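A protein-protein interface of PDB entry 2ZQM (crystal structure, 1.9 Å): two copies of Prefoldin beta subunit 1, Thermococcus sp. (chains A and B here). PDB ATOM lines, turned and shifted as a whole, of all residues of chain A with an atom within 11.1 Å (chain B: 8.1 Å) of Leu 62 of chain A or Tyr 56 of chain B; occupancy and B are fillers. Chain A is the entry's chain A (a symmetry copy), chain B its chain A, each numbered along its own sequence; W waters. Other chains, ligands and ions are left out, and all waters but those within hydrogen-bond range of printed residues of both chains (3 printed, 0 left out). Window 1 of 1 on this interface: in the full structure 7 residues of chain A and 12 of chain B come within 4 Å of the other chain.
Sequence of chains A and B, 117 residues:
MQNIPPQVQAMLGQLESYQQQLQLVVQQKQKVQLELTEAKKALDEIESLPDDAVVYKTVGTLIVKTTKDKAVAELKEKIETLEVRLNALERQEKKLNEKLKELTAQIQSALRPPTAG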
ATOM      1  N   VAL A  54      33.489  15.028   5.142  1.00  0.00           N
ATOM      2  CA  VAL A  54      32.245  15.218   4.404  1.00  0.00           C
ATOM      3  C   VAL A  54      32.451  14.743   2.956  1.00  0.00           C
ATOM      4  O   VAL A  54      33.441  15.104   2.312  1.00  0.00           O
ATOM      5  CB  VAL A  54      31.820  16.708   4.403  1.00  0.00           C
ATOM      6  CG1 VAL A  54      32.889  17.561   3.737  1.00  0.00           C
ATOM      7  CG2 VAL A  54      30.484  16.864   3.694  1.00  0.00           C
ATOM      8  N   VAL A  55      31.534  13.921   2.448  1.00  0.00           N
ATOM      9  CA  VAL A  55      31.649  13.419   1.083  1.00  0.00           C
ATOM     10  C   VAL A  55      30.311  13.494   0.345  1.00  0.00           C
ATOM     11  O   VAL A  55      29.277  13.137   0.897  1.00  0.00           O
ATOM     12  CB  VAL A  55      32.138  11.931   1.058  1.00  0.00           C
ATOM     13  CG1 VAL A  55      32.312  11.461  -0.383  1.00  0.00           C
ATOM     14  CG2 VAL A  55      33.448  11.784   1.810  1.00  0.00           C
ATOM     15  N   TYR A  56      30.342  13.970  -0.902  1.00  0.00           N
ATOM     16  CA  TYR A  56      29.146  14.045  -1.752  1.00  0.00           C
ATOM     17  C   TYR A  56      29.439  13.189  -2.978  1.00  0.00           C
ATOM     18  O   TYR A  56      30.590  13.000  -3.345  1.00  0.00           O
ATOM     19  CB  TYR A  56      28.876  15.484  -2.230  1.00  0.00           C
ATOM     20  CG  TYR A  56      28.460  16.439  -1.137  1.00  0.00           C
ATOM     21  CD1 TYR A  56      27.114  16.695  -0.879  1.00  0.00           C
ATOM     22  CD2 TYR A  56      29.416  17.050  -0.326  1.00  0.00           C
ATOM     23  CE1 TYR A  56      26.731  17.540   0.171  1.00  0.00           C
ATOM     24  CE2 TYR A  56      29.046  17.889   0.720  1.00  0.00           C
ATOM     25  CZ  TYR A  56      27.703  18.126   0.964  1.00  0.00           C
ATOM     26  OH  TYR A  56      27.348  18.949   2.013  1.00  0.00           O
ATOM     27  N   LYS A  57      28.404  12.673  -3.619  1.00  0.00           N
ATOM     28  CA  LYS A  57      28.619  11.876  -4.814  1.00  0.00           C
ATOM     29  C   LYS A  57      27.718  12.411  -5.913  1.00  0.00           C
ATOM     30  O   LYS A  57      26.703  13.043  -5.638  1.00  0.00           O
ATOM     31  CB  LYS A  57      28.311  10.392  -4.561  1.00  0.00           C
ATOM     32  CG  LYS A  57      26.880  10.100  -4.140  1.00  0.00           C
ATOM     33  CD  LYS A  57      26.608   8.592  -4.090  1.00  0.00           C
ATOM     34  CE  LYS A  57      26.713   7.961  -5.480  1.00  0.00           C
ATOM     35  NZ  LYS A  57      26.332   6.500  -5.504  1.00  0.00           N
ATOM     36  N   THR A  58      28.094  12.162  -7.161  1.00  0.00           N
ATOM     37  CA  THR A  58      27.290  12.632  -8.274  1.00  0.00           C
ATOM     38  C   THR A  58      26.400  11.502  -8.764  1.00  0.00           C
ATOM     39  O   THR A  58      26.810  10.339  -8.794  1.00  0.00           O
ATOM     40  CB  THR A  58      28.172  13.128  -9.444  1.00  0.00           C
ATOM     41  OG1 THR A  58      29.080  12.092  -9.828  1.00  0.00           O
ATOM     42  CG2 THR A  58      28.969  14.358  -9.040  1.00  0.00           C
ATOM     43  N   VAL A  59      25.162  11.847  -9.106  1.00  0.00           N
ATOM     44  CA  VAL A  59      24.200  10.882  -9.634  1.00  0.00           C
ATOM     45  C   VAL A  59      23.697  11.584 -10.882  1.00  0.00           C
ATOM     46  O   VAL A  59      22.756  12.383 -10.832  1.00  0.00           O
ATOM     47  CB  VAL A  59      23.035  10.645  -8.659  1.00  0.00           C
ATOM     48  CG1 VAL A  59      22.041   9.653  -9.278  1.00  0.00           C
ATOM     49  CG2 VAL A  59      23.570  10.111  -7.323  1.00  0.00           C
ATOM     50  N   GLY A  60      24.349  11.312 -12.000  1.00  0.00           N
ATOM     51  CA  GLY A  60      23.976  11.988 -13.227  1.00  0.00           C
ATOM     52  C   GLY A  60      24.368  13.445 -13.053  1.00  0.00           C
ATOM     53  O   GLY A  60      25.512  13.760 -12.732  1.00  0.00           O
ATOM     54  N   THR A  61      23.413  14.345 -13.240  1.00  0.00           N
ATOM     55  CA  THR A  61      23.688  15.766 -13.092  1.00  0.00           C
ATOM     56  C   THR A  61      23.394  16.220 -11.664  1.00  0.00           C
ATOM     57  O   THR A  61      23.471  17.403 -11.360  1.00  0.00           O
ATOM     58  CB  THR A  61      22.814  16.605 -14.049  1.00  0.00           C
ATOM     59  OG1 THR A  61      21.434  16.459 -13.687  1.00  0.00           O
ATOM     60  CG2 THR A  61      22.999  16.145 -15.472  1.00  0.00           C
ATOM     61  N   LEU A  62      23.051  15.282 -10.787  1.00  0.00           N
ATOM     62  CA  LEU A  62      22.731  15.636  -9.408  1.00  0.00           C
ATOM     63  C   LEU A  62      23.881  15.347  -8.446  1.00  0.00           C
ATOM     64  O   LEU A  62      24.782  14.567  -8.743  1.00  0.00           O
ATOM     65  CB  LEU A  62      21.479  14.883  -8.959  1.00  0.00           C
ATOM     66  CG  LEU A  62      20.323  15.138  -9.929  1.00  0.00           C
ATOM     67  CD1 LEU A  62      19.261  14.076  -9.779  1.00  0.00           C
ATOM     68  CD2 LEU A  62      19.756  16.509  -9.678  1.00  0.00           C
ATOM     69  N   ILE A  63      23.834  15.989  -7.290  1.00  0.00           N
ATOM     70  CA  ILE A  63      24.858  15.810  -6.274  1.00  0.00           C
ATOM     71  C   ILE A  63      24.160  15.558  -4.955  1.00  0.00           C
ATOM     72  O   ILE A  63      23.332  16.353  -4.529  1.00  0.00           O
ATOM     73  CB  ILE A  63      25.745  17.068  -6.170  1.00  0.00           C
ATOM     74  CG1 ILE A  63      26.532  17.233  -7.478  1.00  0.00           C
ATOM     75  CG2 ILE A  63      26.670  16.972  -4.930  1.00  0.00           C
ATOM     76  CD1 ILE A  63      27.179  18.597  -7.667  1.00  0.00           C
ATOM     77  N   VAL A  64      24.459  14.426  -4.322  1.00  0.00           N
ATOM     78  CA  VAL A  64      23.848  14.115  -3.032  1.00  0.00           C
ATOM     79  C   VAL A  64      24.910  13.771  -1.995  1.00  0.00           C
ATOM     80  O   VAL A  64      26.044  13.415  -2.328  1.00  0.00           O
ATOM     81  CB  VAL A  64      22.853  12.947  -3.143  1.00  0.00           C
ATOM     82  CG1 VAL A  64      21.723  13.334  -4.087  1.00  0.00           C
ATOM     83  CG2 VAL A  64      23.560  11.706  -3.632  1.00  0.00           C
ATOM     84  N   LYS A  65      24.548  13.889  -0.731  1.00  0.00           N
ATOM     85  CA  LYS A  65      25.515  13.610   0.305  1.00  0.00           C
ATOM     86  C   LYS A  65      25.675  12.099   0.470  1.00  0.00           C
ATOM     87  O   LYS A  65      24.728  11.340   0.284  1.00  0.00           O
ATOM     88  CB  LYS A  65      25.068  14.254   1.620  1.00  0.00           C
ATOM     89  CG  LYS A  65      26.208  14.477   2.617  1.00  0.00           C
ATOM     90  CD  LYS A  65      25.702  14.960   3.970  1.00  0.00           C
ATOM     91  CE  LYS A  65      24.956  16.278   3.866  1.00  0.00           C
ATOM     92  NZ  LYS A  65      25.837  17.413   3.479  1.00  0.00           N
ATOM     93  N   THR A  66      26.892  11.658   0.755  1.00  0.00           N
ATOM     94  CA  THR A  66      27.136  10.243   1.013  1.00  0.00           C
ATOM     95  C   THR A  66      28.074  10.229   2.209  1.00  0.00           C
ATOM     96  O   THR A  66      28.084  11.200   2.968  1.00  0.00           O
ATOM     97  CB  THR A  66      27.759   9.513  -0.210  1.00  0.00           C
ATOM     98  OG1 THR A  66      27.926   8.126   0.111  1.00  0.00           O
ATOM     99  CG2 THR A  66      29.100  10.103  -0.600  1.00  0.00           C
ATOM    100  N   ALA B  42      19.584   6.619 -12.647  1.00  0.00           N
ATOM    101  CA  ALA B  42      19.669   7.808 -11.813  1.00  0.00           C
ATOM    102  C   ALA B  42      18.360   8.035 -11.043  1.00  0.00           C
ATOM    103  O   ALA B  42      18.376   8.392  -9.869  1.00  0.00           O
ATOM    104  CB  ALA B  42      19.984   9.024 -12.682  1.00  0.00           C
ATOM    105  N   LEU B  43      17.224   7.843 -11.709  1.00  0.00           N
ATOM    106  CA  LEU B  43      15.928   8.035 -11.055  1.00  0.00           C
ATOM    107  C   LEU B  43      15.736   7.016  -9.938  1.00  0.00           C
ATOM    108  O   LEU B  43      15.227   7.333  -8.858  1.00  0.00           O
ATOM    109  CB  LEU B  43      14.789   7.880 -12.064  1.00  0.00           C
ATOM    110  CG  LEU B  43      13.374   7.867 -11.476  1.00  0.00           C
ATOM    111  CD1 LEU B  43      13.098   9.175 -10.749  1.00  0.00           C
ATOM    112  CD2 LEU B  43      12.353   7.648 -12.583  1.00  0.00           C
ATOM    113  N   GLU B  45      18.005   5.553  -8.196  1.00  0.00           N
ATOM    114  CA  GLU B  45      18.832   5.962  -7.077  1.00  0.00           C
ATOM    115  C   GLU B  45      18.299   7.159  -6.324  1.00  0.00           C
ATOM    116  O   GLU B  45      18.310   7.173  -5.095  1.00  0.00           O
ATOM    117  CB  GLU B  45      20.265   6.236  -7.549  1.00  0.00           C
ATOM    118  CG  GLU B  45      21.119   6.949  -6.505  1.00  0.00           C
ATOM    119  CD  GLU B  45      22.595   6.586  -6.585  1.00  0.00           C
ATOM    120  OE1 GLU B  45      23.049   6.115  -7.653  1.00  0.00           O
ATOM    121  OE2 GLU B  45      23.301   6.784  -5.574  1.00  0.00           O
ATOM    122  N   ILE B  46      17.817   8.170  -7.036  1.00  0.00           N
ATOM    123  CA  ILE B  46      17.304   9.344  -6.344  1.00  0.00           C
ATOM    124  C   ILE B  46      16.018   8.989  -5.595  1.00  0.00           C
ATOM    125  O   ILE B  46      15.767   9.483  -4.500  1.00  0.00           O
ATOM    126  CB  ILE B  46      17.038  10.520  -7.330  1.00  0.00           C
ATOM    127  CG1 ILE B  46      18.371  10.991  -7.935  1.00  0.00           C
ATOM    128  CG2 ILE B  46      16.308  11.671  -6.617  1.00  0.00           C
ATOM    129  CD1 ILE B  46      19.379  11.499  -6.917  1.00  0.00           C
ATOM    130  N   GLU B  47      15.203   8.127  -6.176  1.00  0.00           N
ATOM    131  CA  GLU B  47      13.966   7.771  -5.511  1.00  0.00           C
ATOM    132  C   GLU B  47      14.200   7.011  -4.209  1.00  0.00           C
ATOM    133  O   GLU B  47      13.350   7.038  -3.317  1.00  0.00           O
ATOM    134  CB  GLU B  47      13.074   6.972  -6.454  1.00  0.00           C
ATOM    135  CG  GLU B  47      12.496   7.854  -7.551  1.00  0.00           C
ATOM    136  CD  GLU B  47      11.437   7.162  -8.366  1.00  0.00           C
ATOM    137  OE1 GLU B  47      11.577   5.950  -8.604  1.00  0.00           O
ATOM    138  OE2 GLU B  47      10.471   7.834  -8.781  1.00  0.00           O
ATOM    139  N   LEU B  49      16.338   7.781  -1.965  1.00  0.00           N
ATOM    140  CA  LEU B  49      16.764   8.713  -0.919  1.00  0.00           C
ATOM    141  C   LEU B  49      15.641   9.111   0.045  1.00  0.00           C
ATOM    142  O   LEU B  49      14.461   9.102  -0.324  1.00  0.00           O
ATOM    143  CB  LEU B  49      17.300   9.999  -1.545  1.00  0.00           C
ATOM    144  CG  LEU B  49      18.497   9.908  -2.489  1.00  0.00           C
ATOM    145  CD1 LEU B  49      18.759  11.274  -3.077  1.00  0.00           C
ATOM    146  CD2 LEU B  49      19.710   9.402  -1.737  1.00  0.00           C
ATOM    147  N   ALA B  53      16.373  14.319   2.054  1.00  0.00           N
ATOM    148  CA  ALA B  53      17.766  14.261   1.630  1.00  0.00           C
ATOM    149  C   ALA B  53      18.152  15.557   0.946  1.00  0.00           C
ATOM    150  O   ALA B  53      17.341  16.152   0.247  1.00  0.00           O
ATOM    151  CB  ALA B  53      17.973  13.102   0.674  1.00  0.00           C
ATOM    152  N   VAL B  54      19.382  16.004   1.163  1.00  0.00           N
ATOM    153  CA  VAL B  54      19.868  17.217   0.514  1.00  0.00           C
ATOM    154  C   VAL B  54      20.258  16.880  -0.934  1.00  0.00           C
ATOM    155  O   VAL B  54      20.963  15.898  -1.183  1.00  0.00           O
ATOM    156  CB  VAL B  54      21.099  17.792   1.260  1.00  0.00           C
ATOM    157  CG1 VAL B  54      22.235  16.779   1.263  1.00  0.00           C
ATOM    158  CG2 VAL B  54      21.536  19.093   0.608  1.00  0.00           C
ATOM    159  N   VAL B  55      19.789  17.678  -1.892  1.00  0.00           N
ATOM    160  CA  VAL B  55      20.105  17.433  -3.295  1.00  0.00           C
ATOM    161  C   VAL B  55      20.491  18.728  -4.015  1.00  0.00           C
ATOM    162  O   VAL B  55      19.835  19.750  -3.846  1.00  0.00           O
ATOM    163  CB  VAL B  55      18.894  16.794  -4.056  1.00  0.00           C
ATOM    164  CG1 VAL B  55      19.283  16.490  -5.499  1.00  0.00           C
ATOM    165  CG2 VAL B  55      18.440  15.521  -3.365  1.00  0.00           C
ATOM    166  N   TYR B  56      21.563  18.674  -4.809  1.00  0.00           N
ATOM    167  CA  TYR B  56      22.016  19.821  -5.607  1.00  0.00           C
ATOM    168  C   TYR B  56      21.970  19.373  -7.063  1.00  0.00           C
ATOM    169  O   TYR B  56      22.073  18.189  -7.353  1.00  0.00           O
ATOM    170  CB  TYR B  56      23.468  20.209  -5.274  1.00  0.00           C
ATOM    171  CG  TYR B  56      23.662  20.784  -3.891  1.00  0.00           C
ATOM    172  CD1 TYR B  56      23.663  22.161  -3.677  1.00  0.00           C
ATOM    173  CD2 TYR B  56      23.793  19.943  -2.786  1.00  0.00           C
ATOM    174  CE1 TYR B  56      23.788  22.689  -2.386  1.00  0.00           C
ATOM    175  CE2 TYR B  56      23.916  20.456  -1.500  1.00  0.00           C
ATOM    176  CZ  TYR B  56      23.910  21.829  -1.307  1.00  0.00           C
ATOM    177  OH  TYR B  56      24.019  22.326  -0.025  1.00  0.00           O
ATOM    178  N   LYS B  57      21.823  20.311  -7.983  1.00  0.00           N
ATOM    179  CA  LYS B  57      21.806  19.947  -9.389  1.00  0.00           C
ATOM    180  C   LYS B  57      22.796  20.833 -10.123  1.00  0.00           C
ATOM    181  O   LYS B  57      23.123  21.922  -9.662  1.00  0.00           O
ATOM    182  CB  LYS B  57      20.404  20.115  -9.994  1.00  0.00           C
ATOM    183  CG  LYS B  57      19.851  21.530  -9.943  1.00  0.00           C
ATOM    184  CD  LYS B  57      18.540  21.648 -10.729  1.00  0.00           C
ATOM    185  CE  LYS B  57      18.762  21.400 -12.222  1.00  0.00           C
ATOM    186  NZ  LYS B  57      17.524  21.627 -13.057  1.00  0.00           N
ATOM    187  N   THR B  58      23.278  20.363 -11.266  1.00  0.00           N
ATOM    188  CA  THR B  58      24.227  21.146 -12.036  1.00  0.00           C
ATOM    189  C   THR B  58      23.489  21.886 -13.140  1.00  0.00           C
ATOM    190  O   THR B  58      22.550  21.358 -13.740  1.00  0.00           O
ATOM    191  CB  THR B  58      25.322  20.254 -12.667  1.00  0.00           C
ATOM    192  OG1 THR B  58      24.707  19.224 -13.445  1.00  0.00           O
ATOM    193  CG2 THR B  58      26.184  19.612 -11.592  1.00  0.00           C
ATOM    194  N   VAL B  59      23.894  23.131 -13.373  1.00  0.00           N
ATOM    195  CA  VAL B  59      23.312  23.957 -14.429  1.00  0.00           C
ATOM    196  C   VAL B  59      24.545  24.457 -15.159  1.00  0.00           C
ATOM    197  O   VAL B  59      25.138  25.476 -14.789  1.00  0.00           O
ATOM    198  CB  VAL B  59      22.524  25.145 -13.854  1.00  0.00           C
ATOM    199  CG1 VAL B  59      21.965  25.996 -15.004  1.00  0.00           C
ATOM    200  CG2 VAL B  59      21.386  24.636 -12.958  1.00  0.00           C
ATOM    201  N   LEU B  62      27.570  25.484 -13.184  1.00  0.00           N
ATOM    202  CA  LEU B  62      27.108  25.916 -11.869  1.00  0.00           C
ATOM    203  C   LEU B  62      26.413  24.800 -11.094  1.00  0.00           C
ATOM    204  O   LEU B  62      25.967  23.808 -11.665  1.00  0.00           O
ATOM    205  CB  LEU B  62      26.164  27.108 -12.019  1.00  0.00           C
ATOM    206  CG  LEU B  62      26.835  28.227 -12.820  1.00  0.00           C
ATOM    207  CD1 LEU B  62      25.801  29.181 -13.366  1.00  0.00           C
ATOM    208  CD2 LEU B  62      27.822  28.945 -11.940  1.00  0.00           C
ATOM    209  N   ILE B  63      26.329  24.978  -9.785  1.00  0.00           N
ATOM    210  CA  ILE B  63      25.690  24.002  -8.920  1.00  0.00           C
ATOM    211  C   ILE B  63      24.730  24.744  -8.015  1.00  0.00           C
ATOM    212  O   ILE B  63      25.124  25.672  -7.321  1.00  0.00           O
ATOM    213  CB  ILE B  63      26.743  23.256  -8.073  1.00  0.00           C
ATOM    214  CG1 ILE B  63      27.629  22.417  -9.005  1.00  0.00           C
ATOM    215  CG2 ILE B  63      26.047  22.398  -6.985  1.00  0.00           C
ATOM    216  CD1 ILE B  63      28.914  21.902  -8.374  1.00  0.00           C
ATOM    217  N   VAL B  64      23.455  24.368  -8.052  1.00  0.00           N
ATOM    218  CA  VAL B  64      22.466  25.017  -7.195  1.00  0.00           C
ATOM    219  C   VAL B  64      21.678  23.986  -6.395  1.00  0.00           C
ATOM    220  O   VAL B  64      21.622  22.804  -6.747  1.00  0.00           O
ATOM    221  CB  VAL B  64      21.487  25.879  -8.010  1.00  0.00           C
ATOM    222  CG1 VAL B  64      22.256  26.986  -8.716  1.00  0.00           C
ATOM    223  CG2 VAL B  64      20.745  25.020  -9.007  1.00  0.00           C
ATOM    224  N   LYS B  65      21.078  24.429  -5.306  1.00  0.00           N
ATOM    225  CA  LYS B  65      20.341  23.500  -4.483  1.00  0.00           C
ATOM    226  C   LYS B  65      18.989  23.196  -5.129  1.00  0.00           C
ATOM    227  O   LYS B  65      18.398  24.048  -5.786  1.00  0.00           O
ATOM    228  CB  LYS B  65      20.151  24.085  -3.081  1.00  0.00           C
ATOM    229  CG  LYS B  65      19.867  23.033  -2.005  1.00  0.00           C
ATOM    230  CD  LYS B  65      19.519  23.663  -0.663  1.00  0.00           C
ATOM    231  CE  LYS B  65      20.642  24.533  -0.129  1.00  0.00           C
ATOM    232  NZ  LYS B  65      21.853  23.753   0.239  1.00  0.00           N
ATOM    233  N   THR B  66      18.534  21.958  -4.997  1.00  0.00           N
ATOM    234  CA  THR B  66      17.217  21.586  -5.505  1.00  0.00           C
ATOM    235  C   THR B  66      16.616  20.721  -4.409  1.00  0.00           C
ATOM    236  O   THR B  66      17.026  20.854  -3.255  1.00  0.00           O
ATOM    237  CB  THR B  66      17.295  20.822  -6.857  1.00  0.00           C
ATOM    238  OG1 THR B  66      15.965  20.532  -7.306  1.00  0.00           O
ATOM    239  CG2 THR B  66      18.077  19.528  -6.733  1.00  0.00           C
ATOM    240  N   THR B  67      15.636  19.873  -4.726  1.00  0.00           N
ATOM    241  CA  THR B  67      15.055  18.992  -3.716  1.00  0.00           C
ATOM    242  C   THR B  67      14.864  17.618  -4.322  1.00  0.00           C
ATOM    243  O   THR B  67      14.952  17.454  -5.540  1.00  0.00           O
ATOM    244  CB  THR B  67      13.654  19.457  -3.209  1.00  0.00           C
ATOM    245  OG1 THR B  67      12.700  19.332  -4.274  1.00  0.00           O
ATOM    246  CG2 THR B  67      13.694  20.902  -2.701  1.00  0.00           C
ATOM    247  N   LYS B  68      14.597  16.626  -3.478  1.00  0.00           N
ATOM    248  CA  LYS B  68      14.385  15.288  -3.988  1.00  0.00           C
ATOM    249  C   LYS B  68      13.231  15.256  -4.976  1.00  0.00           C
ATOM    250  O   LYS B  68      13.375  14.721  -6.076  1.00  0.00           O
ATOM    251  CB  LYS B  68      14.098  14.296  -2.865  1.00  0.00           C
ATOM    252  CG  LYS B  68      13.791  12.900  -3.390  1.00  0.00           C
ATOM    253  CD  LYS B  68      13.394  11.926  -2.282  1.00  0.00           C
ATOM    254  CE  LYS B  68      13.006  10.575  -2.867  1.00  0.00           C
ATOM    255  NZ  LYS B  68      12.471   9.618  -1.850  1.00  0.00           N
ATOM    256  N   LYS B  70      11.887  17.612  -6.819  1.00  0.00           N
ATOM    257  CA  LYS B  70      12.146  18.302  -8.071  1.00  0.00           C
ATOM    258  C   LYS B  70      13.083  17.511  -8.983  1.00  0.00           C
ATOM    259  O   LYS B  70      12.898  17.466 -10.204  1.00  0.00           O
ATOM    260  CB  LYS B  70      12.714  19.685  -7.780  1.00  0.00           C
ATOM    261  CG  LYS B  70      11.716  20.583  -7.081  1.00  0.00           C
ATOM    262  CD  LYS B  70      12.372  21.864  -6.585  1.00  0.00           C
ATOM    263  CE  LYS B  70      11.365  22.752  -5.870  1.00  0.00           C
ATOM    264  NZ  LYS B  70      12.033  23.892  -5.178  1.00  0.00           N
ATOM    265  N   ALA B  71      14.095  16.883  -8.403  1.00  0.00           N
ATOM    266  CA  ALA B  71      15.031  16.105  -9.208  1.00  0.00           C
ATOM    267  C   ALA B  71      14.331  14.890  -9.811  1.00  0.00           C
ATOM    268  O   ALA B  71      14.580  14.519 -10.961  1.00  0.00           O
ATOM    269  CB  ALA B  71      16.202  15.670  -8.352  1.00  0.00           C
ATOM    270  N   VAL B  72      13.467  14.266  -9.021  1.00  0.00           N
ATOM    271  CA  VAL B  72      12.712  13.099  -9.471  1.00  0.00           C
ATOM    272  C   VAL B  72      11.836  13.518 -10.658  1.00  0.00           C
ATOM    273  O   VAL B  72      11.830  12.864 -11.688  1.00  0.00           O
ATOM    274  CB  VAL B  72      11.830  12.552  -8.315  1.00  0.00           C
ATOM    275  CG1 VAL B  72      10.744  11.581  -8.846  1.00  0.00           C
ATOM    276  CG2 VAL B  72      12.721  11.822  -7.312  1.00  0.00           C
ATOM    277  N   GLU B  74      12.164  16.076 -12.760  1.00  0.00           N
ATOM    278  CA  GLU B  74      12.970  16.388 -13.927  1.00  0.00           C
ATOM    279  C   GLU B  74      13.516  15.119 -14.584  1.00  0.00           C
ATOM    280  O   GLU B  74      13.657  15.070 -15.799  1.00  0.00           O
ATOM    281  CB  GLU B  74      14.105  17.345 -13.533  1.00  0.00           C
ATOM    282  CG  GLU B  74      13.602  18.750 -13.192  1.00  0.00           C
ATOM    283  CD  GLU B  74      14.702  19.699 -12.741  1.00  0.00           C
ATOM    284  OE1 GLU B  74      15.714  19.821 -13.458  1.00  0.00           O
ATOM    285  OE2 GLU B  74      14.550  20.334 -11.674  1.00  0.00           O
ATOM    286  N   LEU B  75      13.810  14.095 -13.788  1.00  0.00           N
ATOM    287  CA  LEU B  75      14.310  12.836 -14.333  1.00  0.00           C
ATOM    288  C   LEU B  75      13.162  12.094 -15.020  1.00  0.00           C
ATOM    289  O   LEU B  75      13.353  11.476 -16.058  1.00  0.00           O
ATOM    290  CB  LEU B  75      14.915  11.961 -13.231  1.00  0.00           C
ATOM    291  CG  LEU B  75      16.396  12.236 -12.964  1.00  0.00           C
ATOM    292  CD1 LEU B  75      16.802  11.602 -11.628  1.00  0.00           C
ATOM    293  CD2 LEU B  75      17.219  11.687 -14.107  1.00  0.00           C
HETATM  294  O   HOH W   1      21.983  13.914   0.124  1.00  0.00           O
HETATM  295  O   HOH W   2      24.524  20.711   2.286  1.00  0.00           O
HETATM  296  O   HOH W   3      25.984   5.610  -8.550  1.00  0.00           O
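The side-chain carboxylate of Glu 45 of chain B lies within salt-bridge range of the side-chain amino group of Lys 57 of chain A (3.0 Å).
The backbone NH (N) of Ile 63 of chain A sits at hydrogen-bond distance from the backbone carbonyl oxygen (O) of Tyr 56 of chain B, at 2.8 Å.
N of Thr 58 of chain B lies within hydrogen-bond range of O of Thr 61 of chain A.
OH of Tyr 56 of chain B lies within hydrogen-bond range of NZ of Lys 65 of chain B, at 2.6 Å.
The backbone carbonyl oxygen (O) of Val 55 of chain B lies within hydrogen-bond range of the backbone NH (N) of Thr 66 of chain B (2.8 Å).
NZ of Lys 57 of chain B lies within salt-bridge range of OE1 of Glu 74 of chain B (2.6 Å).
The backbone NH of Lys 57 of chain A lies within hydrogen-bond range of the backbone carbonyl oxygen of Val 64 of chain A, 2.8 Å away.
CG1 of Val 59 of chain A touches O of Ala 42 of chain B (3.9 Å).
Val 59 of chain A touches Glu 45 of chain B (CG2 to CD, 3.7 Å).
Lys 57 of chain B touches Thr 61 of chain A (CA to O, 3.6 Å).
Ile 46 of chain B touches Leu 62 of chain A (CG1 to CD1, 3.7 Å).
O of Tyr 56 of chain B touches CA of Leu 62 of chain A, 3.3 Å away.
CB of Ala 71 of chain B touches CD1 of Leu 62 of chain A, 3.7 Å away.
Leu 75 of chain B touches Leu 62 of chain A (CD1 to CD1, 3.9 Å).
Val 54 of chain B touches Val 64 of chain A (O to CA, 3.9 Å).
Val 54 of chain B touches Lys 65 of chain A.
Leu 62 of chain A touches just these residues of chain B: Ile 46 (3.7 Å), Tyr 56 (3.3 Å), Lys 57 (3.7 Å), Ala 71 (3.7 Å) and Leu 75 (3.9 Å).
Tyr 56 of chain B touches two residues of chain A.
Val 54 of chain B touches two residues of chain A.
Of chain A, only Thr 61 (3.6 Å) and Leu 62 (3.7 Å) come within 4 Å of Lys 57 of chain B.
Of the printed residues of chain A, Thr 58 of chain B touches Thr 61.
No residue of chain A comes within 4 Å of Lys 65 of chain B.
No residue of chain A comes within 4 Å of Thr 66 of chain B.
Printed residues of chain B within 4 Å of Val 59 of chain A: Ala 42 (3.9 Å) and Glu 45 (3.7 Å).
Printed residues of chain A within 4 Å of Ile 46 of chain B: Leu 62 (3.7 Å).
Printed residues of chain B within 4 Å of Lys 65 of chain A: Val 54.
Printed residues of chain A within 4 Å of Glu 45 of chain B: Lys 57 (3.0 Å) and Val 59 (3.7 Å).
Leu 62 of chain B touches none of the printed residues of chain A.
The nearest residue of chain A that does not touch Tyr 56 of chain B is Thr 61 of chain A (4.3 Å).
Of the 13 printed residues of chain A, 7 touch a printed residue of chain B.
Hydrophobic or aromatic side chains of chain A that line the printed part of chain B: Val 59, Leu 62, Ile 63 and Val 64.
Among the printed residues, 16 pairs touch across the chains.
Among the printed residues, Asp or Glu carboxylates within 4 Å of a Lys or Arg side-chain nitrogen of the other chain: Lys 57 of chain A with Glu 45 of chain B (3.0 Å).
Ile 63 of chain A touches Tyr 56 of chain B, but with the chains exchanged Tyr 56 of chain A does not touch Ile 63 of chain B (8.4 Å).
Ile 63 of chain A touches its own counterpart, Ile 63 of chain B.
Lys 65 of chain A touches Val 54 of chain B, but with the chains exchanged Val 54 of chain A does not touch Lys 65 of chain B (11.6 Å).
Of the 16 pairs that touch across the chains among the printed residues, 1 has its exchanged pair printed and touching as well.
Water W1 bridges the backbone carbonyl oxygen of Val 54 of chain B (2.6 Å) and the backbone NH of Lys 65 of chain A (2.7 Å).
Water W2 lies within hydrogen-bond range of the side-chain hydroxyl (OH) of Tyr 56 of chain B and the side-chain hydroxyl (OH) of Tyr 56 of chain A.
Water W3 lies within hydrogen-bond range of OE1 of Glu 45 of chain B (3.1 Å) and NZ of Lys 57 of chain A (3.2 Å).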
